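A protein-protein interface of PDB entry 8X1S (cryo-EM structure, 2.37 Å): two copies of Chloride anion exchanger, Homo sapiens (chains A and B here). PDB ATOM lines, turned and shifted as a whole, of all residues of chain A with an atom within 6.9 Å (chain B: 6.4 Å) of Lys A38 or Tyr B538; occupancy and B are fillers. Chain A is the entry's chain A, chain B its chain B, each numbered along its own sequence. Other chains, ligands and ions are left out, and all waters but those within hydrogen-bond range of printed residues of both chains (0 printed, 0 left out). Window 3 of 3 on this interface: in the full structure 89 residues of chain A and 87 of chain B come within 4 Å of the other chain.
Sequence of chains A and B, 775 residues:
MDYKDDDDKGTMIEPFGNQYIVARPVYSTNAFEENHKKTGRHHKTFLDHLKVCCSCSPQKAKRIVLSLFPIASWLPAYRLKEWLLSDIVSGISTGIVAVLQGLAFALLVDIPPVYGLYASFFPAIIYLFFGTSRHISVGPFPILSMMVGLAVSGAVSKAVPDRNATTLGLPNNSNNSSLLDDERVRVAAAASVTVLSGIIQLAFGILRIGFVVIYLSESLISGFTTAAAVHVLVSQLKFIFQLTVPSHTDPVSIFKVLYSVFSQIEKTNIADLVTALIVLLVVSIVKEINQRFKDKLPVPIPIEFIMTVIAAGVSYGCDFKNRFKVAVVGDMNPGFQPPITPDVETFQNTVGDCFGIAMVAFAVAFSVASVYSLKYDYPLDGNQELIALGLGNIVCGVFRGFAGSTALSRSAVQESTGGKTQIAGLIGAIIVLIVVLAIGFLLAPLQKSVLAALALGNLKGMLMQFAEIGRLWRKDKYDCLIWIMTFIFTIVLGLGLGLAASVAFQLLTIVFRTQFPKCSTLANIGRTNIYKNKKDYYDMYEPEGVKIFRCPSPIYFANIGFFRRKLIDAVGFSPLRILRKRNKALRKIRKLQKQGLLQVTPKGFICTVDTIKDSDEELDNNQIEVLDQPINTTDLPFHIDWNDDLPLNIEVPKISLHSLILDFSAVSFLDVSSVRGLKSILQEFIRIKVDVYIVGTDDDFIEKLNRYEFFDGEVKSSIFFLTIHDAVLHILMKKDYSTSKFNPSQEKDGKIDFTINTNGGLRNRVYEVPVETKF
The backbone carbonyl oxygen of Asp B536 lies within hydrogen-bond range of the backbone NH of Thr A39 (2.8 Å). The side-chain hydroxyl of Tyr B537 lies within hydrogen-bond range of the side-chain carboxylate of Asp A699 (2.6 Å). The side-chain amino group of Lys A38 lies within salt-bridge range of the side-chain carboxylate of Asp B536. The side-chain carboxylate of Glu A33 sits at hydrogen-bond distance from the side-chain hydroxyl of Tyr B537 (3.0 Å).
SD of Met B540 is in hydrogen-bond range of N of Tyr B537, 3.7 Å away. OD2 of Asp A699 lies within salt-bridge range of NZ of Lys A38 (2.7 Å).
Among the printed residues, merely in contact across the chains: Lys A38 with Tyr B538 (3.0 Å), Lys A38 with Tyr B537 (3.5 Å), Thr A39 with Tyr B537 (3.5 Å), Lys A37 with Tyr B538 (3.5 Å), Lys A37 with Tyr B537 (3.7 Å), His A36 with Ile B525 (3.8 Å), Thr A39 with Tyr B538 (3.9 Å) and His A36 with Tyr B537 (3.95 Å).
Of the printed residues of chain B, Lys A38 touches Asp B536 (3.3 Å), Tyr B537 (3.5 Å) and Tyr B538 (3.0 Å). Of the printed residues of chain A, Tyr B538 touches Lys A37 (3.5 Å), Lys A38 (3.0 Å) and Thr A39 (3.9 Å). Of the printed residues of chain B, His A36 touches Ile B525 and Tyr B537. Of the printed residues of chain B, Asp A699 touches Tyr B537. Of the printed residues of chain B, Lys A37 touches Tyr B537 and Tyr B538. The nearest residue of chain B that does not touch Lys A38 is Lys B532 (6.3 Å).
Of the 7 printed residues of chain B, 4 touch a printed residue of chain A. Printed residues of chain A that touch a printed residue of chain B: Glu A33, His A36, Lys A37, Lys A38, Thr A39 and Asp A699. Hydrophobic or aromatic side chains of chain A within 4 Å of the printed part of chain B: His A36. Among the printed residues, 12 pairs touch across the chains.
No position is printed for both chains.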
ATOM      1  N   GLU A  33       6.716  36.301  29.877  1.00  0.00           N
ATOM      2  CA  GLU A  33       6.430  35.891  28.508  1.00  0.00           C
ATOM      3  C   GLU A  33       6.876  36.939  27.499  1.00  0.00           C
ATOM      4  O   GLU A  33       7.277  36.592  26.386  1.00  0.00           O
ATOM      5  CB  GLU A  33       4.940  35.614  28.316  1.00  0.00           C
ATOM      6  CG  GLU A  33       4.301  34.659  29.308  1.00  0.00           C
ATOM      7  CD  GLU A  33       5.188  33.497  29.695  1.00  0.00           C
ATOM      8  OE1 GLU A  33       5.453  33.326  30.903  1.00  0.00           O
ATOM      9  OE2 GLU A  33       5.620  32.755  28.786  1.00  0.00           O
ATOM     10  N   HIS A  36      10.823  36.579  27.230  1.00  0.00           N
ATOM     11  CA  HIS A  36      11.350  35.281  26.848  1.00  0.00           C
ATOM     12  C   HIS A  36      10.459  34.655  25.796  1.00  0.00           C
ATOM     13  O   HIS A  36       9.303  34.325  26.063  1.00  0.00           O
ATOM     14  CB  HIS A  36      11.465  34.363  28.060  1.00  0.00           C
ATOM     15  CG  HIS A  36      12.421  34.863  29.088  1.00  0.00           C
ATOM     16  ND1 HIS A  36      12.060  35.767  30.060  1.00  0.00           N
ATOM     17  CD2 HIS A  36      13.738  34.623  29.268  1.00  0.00           C
ATOM     18  CE1 HIS A  36      13.109  36.045  30.808  1.00  0.00           C
ATOM     19  NE2 HIS A  36      14.141  35.364  30.349  1.00  0.00           N
ATOM     20  N   LYS A  37      11.005  34.490  24.598  1.00  0.00           N
ATOM     21  CA  LYS A  37      10.194  34.029  23.493  1.00  0.00           C
ATOM     22  C   LYS A  37       9.765  32.584  23.721  1.00  0.00           C
ATOM     23  O   LYS A  37      10.541  31.732  24.150  1.00  0.00           O
ATOM     24  CB  LYS A  37      10.955  34.166  22.180  1.00  0.00           C
ATOM     25  CG  LYS A  37      10.044  34.198  20.974  1.00  0.00           C
ATOM     26  CD  LYS A  37      10.818  34.130  19.677  1.00  0.00           C
ATOM     27  CE  LYS A  37      10.125  33.208  18.693  1.00  0.00           C
ATOM     28  NZ  LYS A  37       8.646  33.412  18.697  1.00  0.00           N
ATOM     29  N   LYS A  38       8.503  32.296  23.441  1.00  0.00           N
ATOM     30  CA  LYS A  38       8.006  30.938  23.601  1.00  0.00           C
ATOM     31  C   LYS A  38       8.333  30.107  22.389  1.00  0.00           C
ATOM     32  O   LYS A  38       8.931  30.594  21.436  1.00  0.00           O
ATOM     33  CB  LYS A  38       6.498  30.947  23.803  1.00  0.00           C
ATOM     34  CG  LYS A  38       6.042  31.209  25.228  1.00  0.00           C
ATOM     35  CD  LYS A  38       5.962  29.913  26.016  1.00  0.00           C
ATOM     36  CE  LYS A  38       5.080  30.070  27.242  1.00  0.00           C
ATOM     37  NZ  LYS A  38       4.829  28.766  27.915  1.00  0.00           N
ATOM     38  N   THR A  39       7.940  28.845  22.419  1.00  0.00           N
ATOM     39  CA  THR A  39       8.180  27.970  21.292  1.00  0.00           C
ATOM     40  C   THR A  39       6.850  27.694  20.624  1.00  0.00           C
ATOM     41  O   THR A  39       5.798  27.853  21.241  1.00  0.00           O
ATOM     42  CB  THR A  39       8.838  26.655  21.729  1.00  0.00           C
ATOM     43  OG1 THR A  39       8.021  26.015  22.715  1.00  0.00           O
ATOM     44  CG2 THR A  39      10.215  26.922  22.311  1.00  0.00           C
ATOM     45  N   GLY A  40       6.884  27.295  19.362  1.00  0.00           N
ATOM     46  CA  GLY A  40       5.658  26.978  18.662  1.00  0.00           C
ATOM     47  C   GLY A  40       4.939  25.821  19.314  1.00  0.00           C
ATOM     48  O   GLY A  40       5.563  24.824  19.682  1.00  0.00           O
ATOM     49  N   ASP A 699       2.223  27.512  33.469  1.00  0.00           N
ATOM     50  CA  ASP A 699       1.636  28.129  32.286  1.00  0.00           C
ATOM     51  C   ASP A 699       0.356  27.435  31.842  1.00  0.00           C
ATOM     52  O   ASP A 699      -0.583  28.100  31.381  1.00  0.00           O
ATOM     53  CB  ASP A 699       2.664  28.120  31.161  1.00  0.00           C
ATOM     54  CG  ASP A 699       3.897  28.931  31.502  1.00  0.00           C
ATOM     55  OD1 ASP A 699       4.118  29.192  32.705  1.00  0.00           O
ATOM     56  OD2 ASP A 699       4.670  29.274  30.587  1.00  0.00           O
ATOM     57  N   ASP A 700       0.310  26.108  31.963  1.00  0.00           N
ATOM     58  CA  ASP A 700      -0.919  25.370  31.707  1.00  0.00           C
ATOM     59  C   ASP A 700      -2.065  25.898  32.549  1.00  0.00           C
ATOM     60  O   ASP A 700      -3.207  25.942  32.086  1.00  0.00           O
ATOM     61  CB  ASP A 700      -0.703  23.894  32.006  1.00  0.00           C
ATOM     62  CG  ASP A 700       0.402  23.289  31.182  1.00  0.00           C
ATOM     63  OD1 ASP A 700       0.191  23.031  29.982  1.00  0.00           O
ATOM     64  OD2 ASP A 700       1.497  23.074  31.737  1.00  0.00           O
ATOM     65  N   ILE B 525      15.729  28.956  32.766  1.00  0.00           N
ATOM     66  CA  ILE B 525      15.617  30.046  31.820  1.00  0.00           C
ATOM     67  C   ILE B 525      16.208  31.285  32.454  1.00  0.00           C
ATOM     68  O   ILE B 525      15.858  31.626  33.580  1.00  0.00           O
ATOM     69  CB  ILE B 525      14.163  30.361  31.466  1.00  0.00           C
ATOM     70  CG1 ILE B 525      13.290  29.117  31.588  1.00  0.00           C
ATOM     71  CG2 ILE B 525      14.068  30.953  30.065  1.00  0.00           C
ATOM     72  CD1 ILE B 525      11.855  29.378  31.201  1.00  0.00           C
ATOM     73  N   LYS B 532      11.330  26.281  34.085  1.00  0.00           N
ATOM     74  CA  LYS B 532      10.054  26.112  33.407  1.00  0.00           C
ATOM     75  C   LYS B 532      10.112  24.909  32.485  1.00  0.00           C
ATOM     76  O   LYS B 532      11.142  24.267  32.338  1.00  0.00           O
ATOM     77  CB  LYS B 532       9.674  27.374  32.633  1.00  0.00           C
ATOM     78  CG  LYS B 532       9.502  28.588  33.506  1.00  0.00           C
ATOM     79  CD  LYS B 532       8.309  29.390  33.110  1.00  0.00           C
ATOM     80  CE  LYS B 532       7.827  30.235  34.256  1.00  0.00           C
ATOM     81  NZ  LYS B 532       7.521  29.399  35.445  1.00  0.00           N
ATOM     82  N   ASP B 536       8.987  24.649  26.314  1.00  0.00           N
ATOM     83  CA  ASP B 536       8.164  25.834  26.128  1.00  0.00           C
ATOM     84  C   ASP B 536       8.932  27.057  25.667  1.00  0.00           C
ATOM     85  O   ASP B 536       8.348  27.917  25.009  1.00  0.00           O
ATOM     86  CB  ASP B 536       7.432  26.174  27.427  1.00  0.00           C
ATOM     87  CG  ASP B 536       6.228  25.301  27.660  1.00  0.00           C
ATOM     88  OD1 ASP B 536       5.953  24.431  26.818  1.00  0.00           O
ATOM     89  OD2 ASP B 536       5.550  25.486  28.690  1.00  0.00           O
ATOM     90  N   TYR B 537      10.214  27.172  25.986  1.00  0.00           N
ATOM     91  CA  TYR B 537      10.967  28.377  25.686  1.00  0.00           C
ATOM     92  C   TYR B 537      12.227  28.026  24.917  1.00  0.00           C
ATOM     93  O   TYR B 537      12.666  26.877  24.889  1.00  0.00           O
ATOM     94  CB  TYR B 537      11.339  29.146  26.960  1.00  0.00           C
ATOM     95  CG  TYR B 537      10.161  29.505  27.818  1.00  0.00           C
ATOM     96  CD1 TYR B 537       9.561  30.742  27.717  1.00  0.00           C
ATOM     97  CD2 TYR B 537       9.642  28.601  28.724  1.00  0.00           C
ATOM     98  CE1 TYR B 537       8.482  31.066  28.493  1.00  0.00           C
ATOM     99  CE2 TYR B 537       8.566  28.915  29.496  1.00  0.00           C
ATOM    100  CZ  TYR B 537       7.992  30.149  29.382  1.00  0.00           C
ATOM    101  OH  TYR B 537       6.910  30.464  30.162  1.00  0.00           O
ATOM    102  N   TYR B 538      12.806  29.040  24.291  1.00  0.00           N
ATOM    103  CA  TYR B 538      14.082  28.888  23.619  1.00  0.00           C
ATOM    104  C   TYR B 538      15.221  29.231  24.567  1.00  0.00           C
ATOM    105  O   TYR B 538      15.058  29.983  25.529  1.00  0.00           O
ATOM    106  CB  TYR B 538      14.161  29.788  22.390  1.00  0.00           C
ATOM    107  CG  TYR B 538      13.277  29.371  21.248  1.00  0.00           C
ATOM    108  CD1 TYR B 538      13.587  28.263  20.479  1.00  0.00           C
ATOM    109  CD2 TYR B 538      12.142  30.094  20.927  1.00  0.00           C
ATOM    110  CE1 TYR B 538      12.784  27.880  19.430  1.00  0.00           C
ATOM    111  CE2 TYR B 538      11.335  29.720  19.881  1.00  0.00           C
ATOM    112  CZ  TYR B 538      11.661  28.612  19.134  1.00  0.00           C
ATOM    113  OH  TYR B 538      10.858  28.230  18.086  1.00  0.00           O
ATOM    114  N   ASP B 539      16.391  28.669  24.275  1.00  0.00           N
ATOM    115  CA  ASP B 539      17.620  28.970  25.005  1.00  0.00           C
ATOM    116  C   ASP B 539      17.517  28.593  26.478  1.00  0.00           C
ATOM    117  O   ASP B 539      18.010  29.306  27.349  1.00  0.00           O
ATOM    118  CB  ASP B 539      18.002  30.444  24.850  1.00  0.00           C
ATOM    119  CG  ASP B 539      18.371  30.797  23.426  1.00  0.00           C
ATOM    120  OD1 ASP B 539      19.002  31.850  23.214  1.00  0.00           O
ATOM    121  OD2 ASP B 539      18.034  30.014  22.514  1.00  0.00           O
ATOM    122  N   MET B 540      16.872  27.473  26.771  1.00  0.00           N
ATOM    123  CA  MET B 540      16.849  26.946  28.122  1.00  0.00           C
ATOM    124  C   MET B 540      18.112  26.137  28.379  1.00  0.00           C
ATOM    125  O   MET B 540      18.885  25.846  27.469  1.00  0.00           O
ATOM    126  CB  MET B 540      15.607  26.093  28.338  1.00  0.00           C
ATOM    127  CG  MET B 540      14.344  26.770  27.877  1.00  0.00           C
ATOM    128  SD  MET B 540      12.855  25.877  28.302  1.00  0.00           S
ATOM    129  CE  MET B 540      12.765  26.215  30.043  1.00  0.00           C
